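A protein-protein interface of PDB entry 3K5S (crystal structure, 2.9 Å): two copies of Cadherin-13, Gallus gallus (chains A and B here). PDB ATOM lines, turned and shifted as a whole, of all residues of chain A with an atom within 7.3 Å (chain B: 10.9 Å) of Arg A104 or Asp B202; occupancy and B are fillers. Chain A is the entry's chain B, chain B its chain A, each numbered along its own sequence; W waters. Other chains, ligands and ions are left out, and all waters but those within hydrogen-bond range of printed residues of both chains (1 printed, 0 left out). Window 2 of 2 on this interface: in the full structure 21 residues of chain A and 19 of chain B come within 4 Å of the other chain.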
ATOM      1  N   ASN A 101     -20.603  10.153  34.708  1.00  0.00           N
ATOM      2  CA  ASN A 101     -21.334   9.263  33.812  1.00  0.00           C
ATOM      3  C   ASN A 101     -20.955   9.466  32.354  1.00  0.00           C
ATOM      4  O   ASN A 101     -21.676  10.112  31.603  1.00  0.00           O
ATOM      5  CB  ASN A 101     -22.836   9.424  33.983  1.00  0.00           C
ATOM      6  CG  ASN A 101     -23.609   8.417  33.181  1.00  0.00           C
ATOM      7  OD1 ASN A 101     -23.018   7.558  32.535  1.00  0.00           O
ATOM      8  ND2 ASN A 101     -24.934   8.511  33.209  1.00  0.00           N
ATOM      9  N   ASP A 102     -19.820   8.908  31.949  1.00  0.00           N
ATOM     10  CA  ASP A 102     -19.293   9.159  30.609  1.00  0.00           C
ATOM     11  C   ASP A 102     -19.148   7.900  29.774  1.00  0.00           C
ATOM     12  O   ASP A 102     -18.344   7.842  28.852  1.00  0.00           O
ATOM     13  CB  ASP A 102     -17.972   9.932  30.670  1.00  0.00           C
ATOM     14  CG  ASP A 102     -16.956   9.279  31.570  1.00  0.00           C
ATOM     15  OD1 ASP A 102     -17.325   8.326  32.291  1.00  0.00           O
ATOM     16  OD2 ASP A 102     -15.789   9.724  31.558  1.00  0.00           O
ATOM     17  N   ASN A 103     -19.942   6.897  30.110  1.00  0.00           N
ATOM     18  CA  ASN A 103     -20.030   5.704  29.295  1.00  0.00           C
ATOM     19  C   ASN A 103     -21.485   5.369  28.997  1.00  0.00           C
ATOM     20  O   ASN A 103     -22.337   5.452  29.875  1.00  0.00           O
ATOM     21  CB  ASN A 103     -19.311   4.530  29.967  1.00  0.00           C
ATOM     22  CG  ASN A 103     -17.793   4.656  29.893  1.00  0.00           C
ATOM     23  OD1 ASN A 103     -17.150   4.102  28.994  1.00  0.00           O
ATOM     24  ND2 ASN A 103     -17.216   5.404  30.829  1.00  0.00           N
ATOM     25  N   ARG A 104     -21.766   5.017  27.744  1.00  0.00           N
ATOM     26  CA  ARG A 104     -23.113   4.640  27.323  1.00  0.00           C
ATOM     27  C   ARG A 104     -23.314   3.118  27.436  1.00  0.00           C
ATOM     28  O   ARG A 104     -22.445   2.345  27.044  1.00  0.00           O
ATOM     29  CB  ARG A 104     -23.347   5.134  25.889  1.00  0.00           C
ATOM     30  CG  ARG A 104     -24.690   4.773  25.277  1.00  0.00           C
ATOM     31  CD  ARG A 104     -24.766   5.173  23.804  1.00  0.00           C
ATOM     32  NE  ARG A 104     -24.741   6.623  23.591  1.00  0.00           N
ATOM     33  CZ  ARG A 104     -25.683   7.473  24.019  1.00  0.00           C
ATOM     34  NH1 ARG A 104     -26.727   7.028  24.713  1.00  0.00           N
ATOM     35  NH2 ARG A 104     -25.579   8.781  23.776  1.00  0.00           N
ATOM     36  N   PRO A 105     -24.458   2.683  27.987  1.00  0.00           N
ATOM     37  CA  PRO A 105     -24.764   1.247  28.052  1.00  0.00           C
ATOM     38  C   PRO A 105     -24.735   0.595  26.669  1.00  0.00           C
ATOM     39  O   PRO A 105     -25.400   1.076  25.750  1.00  0.00           O
ATOM     40  CB  PRO A 105     -26.196   1.220  28.598  1.00  0.00           C
ATOM     41  CG  PRO A 105     -26.352   2.485  29.329  1.00  0.00           C
ATOM     42  CD  PRO A 105     -25.529   3.498  28.579  1.00  0.00           C
ATOM     43  N   MET A 106     -23.985  -0.486  26.516  1.00  0.00           N
ATOM     44  CA  MET A 106     -23.940  -1.165  25.224  1.00  0.00           C
ATOM     45  C   MET A 106     -23.958  -2.698  25.290  1.00  0.00           C
ATOM     46  O   MET A 106     -23.188  -3.313  26.032  1.00  0.00           O
ATOM     47  CB  MET A 106     -22.756  -0.665  24.383  1.00  0.00           C
ATOM     48  CG  MET A 106     -21.567  -0.158  25.195  1.00  0.00           C
ATOM     49  SD  MET A 106     -20.136   0.246  24.169  1.00  0.00           S
ATOM     50  CE  MET A 106     -20.901   1.245  22.887  1.00  0.00           C
ATOM     51  N   PHE A 107     -24.845  -3.299  24.496  1.00  0.00           N
ATOM     52  CA  PHE A 107     -24.899  -4.751  24.336  1.00  0.00           C
ATOM     53  C   PHE A 107     -23.714  -5.281  23.511  1.00  0.00           C
ATOM     54  O   PHE A 107     -23.333  -4.681  22.513  1.00  0.00           O
ATOM     55  CB  PHE A 107     -26.223  -5.144  23.685  1.00  0.00           C
ATOM     56  CG  PHE A 107     -27.419  -4.921  24.564  1.00  0.00           C
ATOM     57  CD1 PHE A 107     -27.821  -5.899  25.471  1.00  0.00           C
ATOM     58  CD2 PHE A 107     -28.147  -3.743  24.484  1.00  0.00           C
ATOM     59  CE1 PHE A 107     -28.925  -5.710  26.291  1.00  0.00           C
ATOM     60  CE2 PHE A 107     -29.258  -3.542  25.304  1.00  0.00           C
ATOM     61  CZ  PHE A 107     -29.646  -4.538  26.210  1.00  0.00           C
ATOM     62  N   PHE A 132     -23.547  -3.928  28.893  1.00  0.00           N
ATOM     63  CA  PHE A 132     -22.317  -3.549  29.582  1.00  0.00           C
ATOM     64  C   PHE A 132     -22.223  -2.036  29.805  1.00  0.00           C
ATOM     65  O   PHE A 132     -22.791  -1.250  29.050  1.00  0.00           O
ATOM     66  CB  PHE A 132     -21.084  -4.053  28.819  1.00  0.00           C
ATOM     67  CG  PHE A 132     -19.782  -3.548  29.378  1.00  0.00           C
ATOM     68  CD1 PHE A 132     -19.254  -4.090  30.542  1.00  0.00           C
ATOM     69  CD2 PHE A 132     -19.093  -2.519  28.751  1.00  0.00           C
ATOM     70  CE1 PHE A 132     -18.063  -3.619  31.069  1.00  0.00           C
ATOM     71  CE2 PHE A 132     -17.903  -2.044  29.267  1.00  0.00           C
ATOM     72  CZ  PHE A 132     -17.386  -2.590  30.430  1.00  0.00           C
ATOM     73  N   ASP A 133     -21.500  -1.638  30.849  1.00  0.00           N
ATOM     74  CA  ASP A 133     -21.303  -0.225  31.160  1.00  0.00           C
ATOM     75  C   ASP A 133     -19.982   0.028  31.876  1.00  0.00           C
ATOM     76  O   ASP A 133     -19.755  -0.469  32.979  1.00  0.00           O
ATOM     77  CB  ASP A 133     -22.456   0.292  32.011  1.00  0.00           C
ATOM     78  CG  ASP A 133     -22.527   1.798  32.029  1.00  0.00           C
ATOM     79  OD1 ASP A 133     -21.468   2.441  32.184  1.00  0.00           O
ATOM     80  OD2 ASP A 133     -23.648   2.331  31.879  1.00  0.00           O
ATOM     81  N   ALA A 134     -19.123   0.825  31.256  1.00  0.00           N
ATOM     82  CA  ALA A 134     -17.768   1.026  31.759  1.00  0.00           C
ATOM     83  C   ALA A 134     -17.664   1.939  32.981  1.00  0.00           C
ATOM     84  O   ALA A 134     -16.561   2.269  33.408  1.00  0.00           O
ATOM     85  CB  ALA A 134     -16.871   1.541  30.651  1.00  0.00           C
ATOM     86  N   ASP A 135     -18.803   2.357  33.528  1.00  0.00           N
ATOM     87  CA  ASP A 135     -18.821   3.241  34.687  1.00  0.00           C
ATOM     88  C   ASP A 135     -18.873   2.421  35.955  1.00  0.00           C
ATOM     89  O   ASP A 135     -18.981   1.203  35.897  1.00  0.00           O
ATOM     90  CB  ASP A 135     -20.030   4.174  34.641  1.00  0.00           C
ATOM     91  CG  ASP A 135     -19.949   5.173  33.508  1.00  0.00           C
ATOM     92  OD1 ASP A 135     -18.839   5.657  33.218  1.00  0.00           O
ATOM     93  OD2 ASP A 135     -20.988   5.478  32.895  1.00  0.00           O
ATOM     94  N   ASN A 141     -24.469   5.603  38.015  1.00  0.00           N
ATOM     95  CA  ASN A 141     -23.835   5.766  36.700  1.00  0.00           C
ATOM     96  C   ASN A 141     -23.607   4.469  35.912  1.00  0.00           C
ATOM     97  O   ASN A 141     -23.306   4.515  34.736  1.00  0.00           O
ATOM     98  CB  ASN A 141     -22.520   6.548  36.812  1.00  0.00           C
ATOM     99  CG  ASN A 141     -22.722   7.992  37.260  1.00  0.00           C
ATOM    100  OD1 ASN A 141     -23.854   8.500  37.340  1.00  0.00           O
ATOM    101  ND2 ASN A 141     -21.619   8.661  37.557  1.00  0.00           N
ATOM    102  N   LEU A 144     -28.173  -0.563  35.618  1.00  0.00           N
ATOM    103  CA  LEU A 144     -29.030  -0.642  34.426  1.00  0.00           C
ATOM    104  C   LEU A 144     -30.490  -1.038  34.681  1.00  0.00           C
ATOM    105  O   LEU A 144     -30.807  -1.867  35.547  1.00  0.00           O
ATOM    106  CB  LEU A 144     -28.419  -1.608  33.405  1.00  0.00           C
ATOM    107  CG  LEU A 144     -26.964  -1.323  33.012  1.00  0.00           C
ATOM    108  CD1 LEU A 144     -26.364  -2.464  32.211  1.00  0.00           C
ATOM    109  CD2 LEU A 144     -26.837  -0.013  32.249  1.00  0.00           C
ATOM    110  N   ALA A 195     -31.470  -0.726  27.225  1.00  0.00           N
ATOM    111  CA  ALA A 195     -30.891  -0.662  28.562  1.00  0.00           C
ATOM    112  C   ALA A 195     -30.621   0.808  28.850  1.00  0.00           C
ATOM    113  O   ALA A 195     -29.982   1.484  28.040  1.00  0.00           O
ATOM    114  CB  ALA A 195     -29.611  -1.453  28.636  1.00  0.00           C
ATOM    115  N   ASP A 197     -29.637   4.110  31.862  1.00  0.00           N
ATOM    116  CA  ASP A 197     -28.770   4.427  33.000  1.00  0.00           C
ATOM    117  C   ASP A 197     -29.532   4.820  34.248  1.00  0.00           C
ATOM    118  O   ASP A 197     -30.768   4.804  34.279  1.00  0.00           O
ATOM    119  CB  ASP A 197     -27.843   5.588  32.651  1.00  0.00           C
ATOM    120  CG  ASP A 197     -26.467   5.135  32.269  1.00  0.00           C
ATOM    121  OD1 ASP A 197     -26.186   3.921  32.354  1.00  0.00           O
ATOM    122  OD2 ASP A 197     -25.659   6.000  31.899  1.00  0.00           O
ATOM    123  N   GLY A 204     -31.452   8.856  32.022  1.00  0.00           N
ATOM    124  CA  GLY A 204     -30.308   7.974  31.867  1.00  0.00           C
ATOM    125  C   GLY A 204     -29.631   8.093  30.509  1.00  0.00           C
ATOM    126  O   GLY A 204     -30.015   8.920  29.689  1.00  0.00           O
ATOM    127  N   LEU A 205     -28.603   7.279  30.289  1.00  0.00           N
ATOM    128  CA  LEU A 205     -28.043   7.072  28.958  1.00  0.00           C
ATOM    129  C   LEU A 205     -28.474   5.694  28.484  1.00  0.00           C
ATOM    130  O   LEU A 205     -28.618   4.779  29.299  1.00  0.00           O
ATOM    131  CB  LEU A 205     -26.517   7.134  28.978  1.00  0.00           C
ATOM    132  CG  LEU A 205     -25.822   8.478  29.176  1.00  0.00           C
ATOM    133  CD1 LEU A 205     -24.362   8.337  28.778  1.00  0.00           C
ATOM    134  CD2 LEU A 205     -26.510   9.561  28.369  1.00  0.00           C
ATOM    135  N   THR A 206     -28.663   5.534  27.173  1.00  0.00           N
ATOM    136  CA  THR A 206     -29.251   4.303  26.638  1.00  0.00           C
ATOM    137  C   THR A 206     -28.393   3.531  25.640  1.00  0.00           C
ATOM    138  O   THR A 206     -27.446   4.053  25.054  1.00  0.00           O
ATOM    139  CB  THR A 206     -30.640   4.550  25.996  1.00  0.00           C
ATOM    140  OG1 THR A 206     -30.564   5.658  25.088  1.00  0.00           O
ATOM    141  CG2 THR A 206     -31.685   4.847  27.063  1.00  0.00           C
ATOM    142  N   GLY A 207     -28.739   2.261  25.478  1.00  0.00           N
ATOM    143  CA  GLY A 207     -28.164   1.408  24.461  1.00  0.00           C
ATOM    144  C   GLY A 207     -29.295   0.519  23.992  1.00  0.00           C
ATOM    145  O   GLY A 207     -30.155   0.144  24.783  1.00  0.00           O
ATOM    146  N   THR A 208     -29.326   0.188  22.711  1.00  0.00           N
ATOM    147  CA  THR A 208     -30.367  -0.706  22.231  1.00  0.00           C
ATOM    148  C   THR A 208     -29.801  -1.909  21.502  1.00  0.00           C
ATOM    149  O   THR A 208     -28.595  -2.027  21.296  1.00  0.00           O
ATOM    150  CB  THR A 208     -31.369   0.018  21.336  1.00  0.00           C
ATOM    151  OG1 THR A 208     -30.673   0.623  20.241  1.00  0.00           O
ATOM    152  CG2 THR A 208     -32.069   1.098  22.121  1.00  0.00           C
ATOM    153  N   ASN B 101     -23.864  14.099  36.329  1.00  0.00           N
ATOM    154  CA  ASN B 101     -24.660  14.553  35.190  1.00  0.00           C
ATOM    155  C   ASN B 101     -26.105  14.023  35.196  1.00  0.00           C
ATOM    156  O   ASN B 101     -26.419  13.052  34.527  1.00  0.00           O
ATOM    157  CB  ASN B 101     -23.963  14.196  33.876  1.00  0.00           C
ATOM    158  CG  ASN B 101     -24.501  14.984  32.697  1.00  0.00           C
ATOM    159  OD1 ASN B 101     -24.807  16.164  32.824  1.00  0.00           O
ATOM    160  ND2 ASN B 101     -24.607  14.337  31.538  1.00  0.00           N
ATOM    161  N   ARG B 104     -30.925  17.056  32.219  1.00  0.00           N
ATOM    162  CA  ARG B 104     -30.798  17.094  30.772  1.00  0.00           C
ATOM    163  C   ARG B 104     -30.917  18.545  30.280  1.00  0.00           C
ATOM    164  O   ARG B 104     -31.730  19.309  30.799  1.00  0.00           O
ATOM    165  CB  ARG B 104     -31.853  16.174  30.146  1.00  0.00           C
ATOM    166  CG  ARG B 104     -32.224  16.502  28.717  1.00  0.00           C
ATOM    167  CD  ARG B 104     -33.623  15.996  28.386  1.00  0.00           C
ATOM    168  NE  ARG B 104     -33.898  14.741  29.074  1.00  0.00           N
ATOM    169  CZ  ARG B 104     -33.477  13.551  28.652  1.00  0.00           C
ATOM    170  NH1 ARG B 104     -32.756  13.460  27.533  1.00  0.00           N
ATOM    171  NH2 ARG B 104     -33.776  12.452  29.347  1.00  0.00           N
ATOM    172  N   ASP B 140     -18.304  19.175  32.880  1.00  0.00           N
ATOM    173  CA  ASP B 140     -18.817  18.854  31.550  1.00  0.00           C
ATOM    174  C   ASP B 140     -20.303  18.571  31.635  1.00  0.00           C
ATOM    175  O   ASP B 140     -20.979  18.444  30.623  1.00  0.00           O
ATOM    176  CB  ASP B 140     -18.133  17.613  30.968  1.00  0.00           C
ATOM    177  CG  ASP B 140     -16.678  17.839  30.637  1.00  0.00           C
ATOM    178  OD1 ASP B 140     -16.236  19.006  30.601  1.00  0.00           O
ATOM    179  OD2 ASP B 140     -15.967  16.839  30.407  1.00  0.00           O
ATOM    180  N   LEU B 143     -22.025  22.651  30.028  1.00  0.00           N
ATOM    181  CA  LEU B 143     -21.069  22.700  28.911  1.00  0.00           C
ATOM    182  C   LEU B 143     -21.716  22.062  27.690  1.00  0.00           C
ATOM    183  O   LEU B 143     -21.509  20.891  27.389  1.00  0.00           O
ATOM    184  CB  LEU B 143     -19.747  21.985  29.223  1.00  0.00           C
ATOM    185  CG  LEU B 143     -18.722  21.892  28.090  1.00  0.00           C
ATOM    186  CD1 LEU B 143     -18.347  23.259  27.547  1.00  0.00           C
ATOM    187  CD2 LEU B 143     -17.493  21.165  28.562  1.00  0.00           C
ATOM    188  N   ARG B 145     -22.981  21.782  23.581  1.00  0.00           N
ATOM    189  CA  ARG B 145     -22.624  22.007  22.189  1.00  0.00           C
ATOM    190  C   ARG B 145     -23.862  21.893  21.309  1.00  0.00           C
ATOM    191  O   ARG B 145     -24.791  21.137  21.610  1.00  0.00           O
ATOM    192  CB  ARG B 145     -21.529  21.051  21.738  1.00  0.00           C
ATOM    193  CG  ARG B 145     -20.211  21.306  22.424  1.00  0.00           C
ATOM    194  CD  ARG B 145     -19.593  22.615  21.969  1.00  0.00           C
ATOM    195  NE  ARG B 145     -18.275  22.836  22.564  1.00  0.00           N
ATOM    196  CZ  ARG B 145     -18.046  23.604  23.629  1.00  0.00           C
ATOM    197  NH1 ARG B 145     -19.045  24.242  24.228  1.00  0.00           N
ATOM    198  NH2 ARG B 145     -16.813  23.739  24.100  1.00  0.00           N
ATOM    199  N   ASN B 147     -26.192  21.677  17.602  1.00  0.00           N
ATOM    200  CA  ASN B 147     -26.300  21.041  16.307  1.00  0.00           C
ATOM    201  C   ASN B 147     -27.676  21.222  15.660  1.00  0.00           C
ATOM    202  O   ASN B 147     -28.695  21.201  16.351  1.00  0.00           O
ATOM    203  CB  ASN B 147     -25.950  19.558  16.442  1.00  0.00           C
ATOM    204  CG  ASN B 147     -25.495  18.940  15.131  1.00  0.00           C
ATOM    205  OD1 ASN B 147     -25.022  19.640  14.235  1.00  0.00           O
ATOM    206  ND2 ASN B 147     -25.634  17.621  15.015  1.00  0.00           N
ATOM    207  N   GLU B 194     -30.574  20.863  18.570  1.00  0.00           N
ATOM    208  CA  GLU B 194     -30.196  19.978  19.653  1.00  0.00           C
ATOM    209  C   GLU B 194     -29.089  20.647  20.453  1.00  0.00           C
ATOM    210  O   GLU B 194     -28.162  21.239  19.885  1.00  0.00           O
ATOM    211  CB  GLU B 194     -29.728  18.631  19.086  1.00  0.00           C
ATOM    212  CG  GLU B 194     -29.177  17.633  20.102  1.00  0.00           C
ATOM    213  CD  GLU B 194     -28.457  16.456  19.423  1.00  0.00           C
ATOM    214  OE1 GLU B 194     -27.390  16.680  18.790  1.00  0.00           O
ATOM    215  OE2 GLU B 194     -28.962  15.303  19.508  1.00  0.00           O
ATOM    216  N   ALA B 195     -29.209  20.599  21.774  1.00  0.00           N
ATOM    217  CA  ALA B 195     -28.091  20.943  22.634  1.00  0.00           C
ATOM    218  C   ALA B 195     -27.589  19.637  23.224  1.00  0.00           C
ATOM    219  O   ALA B 195     -28.393  18.778  23.592  1.00  0.00           O
ATOM    220  CB  ALA B 195     -28.523  21.904  23.724  1.00  0.00           C
ATOM    221  N   LYS B 196     -26.270  19.474  23.294  1.00  0.00           N
ATOM    222  CA  LYS B 196     -25.692  18.255  23.860  1.00  0.00           C
ATOM    223  C   LYS B 196     -24.732  18.539  25.030  1.00  0.00           C
ATOM    224  O   LYS B 196     -23.956  19.491  25.004  1.00  0.00           O
ATOM    225  CB  LYS B 196     -24.993  17.447  22.762  1.00  0.00           C
ATOM    226  CG  LYS B 196     -24.903  15.952  23.021  1.00  0.00           C
ATOM    227  CD  LYS B 196     -24.727  15.174  21.715  1.00  0.00           C
ATOM    228  CE  LYS B 196     -24.782  13.675  21.976  1.00  0.00           C
ATOM    229  NZ  LYS B 196     -24.428  12.849  20.787  1.00  0.00           N
ATOM    230  N   ASP B 197     -24.815  17.703  26.058  1.00  0.00           N
ATOM    231  CA  ASP B 197     -23.933  17.763  27.227  1.00  0.00           C
ATOM    232  C   ASP B 197     -22.499  17.356  26.938  1.00  0.00           C
ATOM    233  O   ASP B 197     -22.164  16.951  25.820  1.00  0.00           O
ATOM    234  CB  ASP B 197     -24.429  16.775  28.274  1.00  0.00           C
ATOM    235  CG  ASP B 197     -25.206  17.427  29.339  1.00  0.00           C
ATOM    236  OD1 ASP B 197     -25.280  18.677  29.332  1.00  0.00           O
ATOM    237  OD2 ASP B 197     -25.728  16.684  30.189  1.00  0.00           O
ATOM    238  N   MET B 198     -21.672  17.412  27.979  1.00  0.00           N
ATOM    239  CA  MET B 198     -20.347  16.814  27.933  1.00  0.00           C
ATOM    240  C   MET B 198     -19.562  17.312  26.723  1.00  0.00           C
ATOM    241  O   MET B 198     -18.790  16.563  26.119  1.00  0.00           O
ATOM    242  CB  MET B 198     -20.448  15.285  27.898  1.00  0.00           C
ATOM    243  CG  MET B 198     -21.428  14.655  28.896  1.00  0.00           C
ATOM    244  SD  MET B 198     -20.841  14.327  30.595  1.00  0.00           S
ATOM    245  CE  MET B 198     -19.065  14.117  30.374  1.00  0.00           C
ATOM    246  N   GLY B 199     -19.776  18.576  26.370  1.00  0.00           N
ATOM    247  CA  GLY B 199     -19.106  19.201  25.243  1.00  0.00           C
ATOM    248  C   GLY B 199     -19.257  18.484  23.914  1.00  0.00           C
ATOM    249  O   GLY B 199     -18.295  18.391  23.145  1.00  0.00           O
ATOM    250  N   GLY B 200     -20.461  17.975  23.655  1.00  0.00           N
ATOM    251  CA  GLY B 200     -20.818  17.378  22.377  1.00  0.00           C
ATOM    252  C   GLY B 200     -20.310  15.969  22.113  1.00  0.00           C
ATOM    253  O   GLY B 200     -20.465  15.442  21.002  1.00  0.00           O
ATOM    254  N   HIS B 201     -19.690  15.357  23.118  1.00  0.00           N
ATOM    255  CA  HIS B 201     -19.206  13.990  22.969  1.00  0.00           C
ATOM    256  C   HIS B 201     -20.394  13.044  23.018  1.00  0.00           C
ATOM    257  O   HIS B 201     -21.434  13.380  23.587  1.00  0.00           O
ATOM    258  CB  HIS B 201     -18.161  13.654  24.034  1.00  0.00           C
ATOM    259  CG  HIS B 201     -17.058  14.662  24.117  1.00  0.00           C
ATOM    260  ND1 HIS B 201     -16.535  15.287  23.005  1.00  0.00           N
ATOM    261  CD2 HIS B 201     -16.378  15.161  25.179  1.00  0.00           C
ATOM    262  CE1 HIS B 201     -15.583  16.123  23.373  1.00  0.00           C
ATOM    263  NE2 HIS B 201     -15.470  16.068  24.690  1.00  0.00           N
ATOM    264  N   ASP B 202     -20.261  11.878  22.398  1.00  0.00           N
ATOM    265  CA  ASP B 202     -21.425  11.025  22.195  1.00  0.00           C
ATOM    266  C   ASP B 202     -22.123  10.640  23.499  1.00  0.00           C
ATOM    267  O   ASP B 202     -23.291  10.266  23.496  1.00  0.00           O
ATOM    268  CB  ASP B 202     -21.074   9.786  21.371  1.00  0.00           C
ATOM    269  CG  ASP B 202     -19.976   8.961  21.997  1.00  0.00           C
ATOM    270  OD1 ASP B 202     -20.161   7.725  22.122  1.00  0.00           O
ATOM    271  OD2 ASP B 202     -18.936   9.551  22.366  1.00  0.00           O
ATOM    272  N   VAL B 203     -21.423  10.750  24.618  1.00  0.00           N
ATOM    273  CA  VAL B 203     -22.041  10.401  25.888  1.00  0.00           C
ATOM    274  C   VAL B 203     -22.884  11.545  26.465  1.00  0.00           C
ATOM    275  O   VAL B 203     -23.164  11.581  27.660  1.00  0.00           O
ATOM    276  CB  VAL B 203     -20.994   9.935  26.926  1.00  0.00           C
ATOM    277  CG1 VAL B 203     -20.445   8.565  26.557  1.00  0.00           C
ATOM    278  CG2 VAL B 203     -19.871  10.949  27.041  1.00  0.00           C
ATOM    279  N   GLY B 204     -23.300  12.473  25.615  1.00  0.00           N
ATOM    280  CA  GLY B 204     -24.068  13.612  26.084  1.00  0.00           C
ATOM    281  C   GLY B 204     -25.557  13.344  26.177  1.00  0.00           C
ATOM    282  O   GLY B 204     -26.090  12.460  25.504  1.00  0.00           O
ATOM    283  N   LEU B 205     -26.231  14.102  27.035  1.00  0.00           N
ATOM    284  CA  LEU B 205     -27.687  14.077  27.097  1.00  0.00           C
ATOM    285  C   LEU B 205     -28.157  15.224  26.229  1.00  0.00           C
ATOM    286  O   LEU B 205     -27.411  16.181  26.009  1.00  0.00           O
ATOM    287  CB  LEU B 205     -28.172  14.258  28.536  1.00  0.00           C
ATOM    288  CG  LEU B 205     -27.935  13.111  29.521  1.00  0.00           C
ATOM    289  CD1 LEU B 205     -27.892  13.645  30.951  1.00  0.00           C
ATOM    290  CD2 LEU B 205     -28.979  12.003  29.363  1.00  0.00           C
ATOM    291  N   THR B 206     -29.371  15.148  25.706  1.00  0.00           N
ATOM    292  CA  THR B 206     -29.759  16.145  24.720  1.00  0.00           C
ATOM    293  C   THR B 206     -31.158  16.680  24.927  1.00  0.00           C
ATOM    294  O   THR B 206     -32.038  15.987  25.413  1.00  0.00           O
ATOM    295  CB  THR B 206     -29.638  15.608  23.289  1.00  0.00           C
ATOM    296  OG1 THR B 206     -30.519  14.495  23.137  1.00  0.00           O
ATOM    297  CG2 THR B 206     -28.220  15.155  22.992  1.00  0.00           C
ATOM    298  N   GLY B 207     -31.340  17.939  24.565  1.00  0.00           N
ATOM    299  CA  GLY B 207     -32.648  18.546  24.565  1.00  0.00           C
ATOM    300  C   GLY B 207     -32.853  19.111  23.186  1.00  0.00           C
ATOM    301  O   GLY B 207     -31.908  19.249  22.424  1.00  0.00           O
HETATM  302  O   HOH W   1     -21.974  12.188  36.215  1.00  0.00           O
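The backbone carbonyl oxygen (O) of Asp B202 is in hydrogen-bond range of the guanidinium group (NH2) of Arg A104, at 2.7 Å.
Of chain B, only Asp B202 (2.7 Å) and Val B203 (3.97 Å) come within 4 Å of Arg A104.
Printed residues of chain A within 4 Å of Asp B202: Arg A104 (2.7 Å).
No residue of chain B comes within 4 Å of Pro A105.
No residue of chain B comes within 4 Å of Met A106.
Leu A205 touches just these residues of chain B: Val B203 and Leu B205.
No residue of chain B comes within 4 Å of Thr A206.
Of the printed residues of chain B, Gly A204 touches Leu B205 (3.3 Å).
Of the printed residues of chain A, Leu B205 touches Gly A204 and Leu A205.
Of the printed residues of chain A, Val B203 touches Asp A102 (3.2 Å), Asn A103 (3.96 Å), Arg A104 (3.97 Å) and Leu A205 (3.6 Å).
Of the printed residues of chain B, Asp A102 touches Val B203.
Asp B197 touches none of the printed residues of chain A.
The nearest printed residue of chain A that does not touch Val B203 is Asn A101 (4.5 Å).
O of Asp A102 touches CG1 of Val B203 (3.2 Å).
Asn A103 touches Val B203.
Val B203 touches Arg A104.
Leu B205 touches Gly A204 (CD2 to O, 3.3 Å).
Val B203 touches Leu A205 (O to CD1, 3.6 Å).
CD2 of Leu B205 touches CD2 of Leu A205, 3.6 Å away.
Of the 20 printed residues of chain B, 3 touch a printed residue of chain A.
Printed residues of chain A that touch a printed residue of chain B: Asp A102, Asn A103, Arg A104, Gly A204 and Leu A205.
Hydrophobic or aromatic side chains of chain A that line the printed part of chain B: Leu A205.
Among the printed residues, 7 pairs touch across the chains.
Among the printed residues, no Asp or Glu carboxylate lies within 4 Å of a Lys or Arg side-chain nitrogen of the other chain.
Water W1 bridges N of Asn B101 (2.7 Å) and N of Asn A101 (2.9 Å).
The backbone carbonyl oxygen (O) of Leu B205 is in hydrogen-bond range of the backbone NH (N) of Asp B197.
The backbone NH (N) of Asp A197 sits at hydrogen-bond distance from the backbone carbonyl oxygen (O) of Leu A205.
The side-chain carboxylate (OD1) of Asp A102 lies close to the side-chain amide nitrogen (ND2) of Asn A103 (3.3 Å).
O of Thr A206 lies close to NH1 of Arg A104 (3.1 Å).
Gly A204 touches Leu B205, but with the chains exchanged Leu A205 does not touch Gly B204 (4.1 Å).
Leu B205 touches its own counterpart, Leu A205.
Of the 7 pairs that touch across the chains among the printed residues, 1 has its exchanged pair printed and touching as well.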
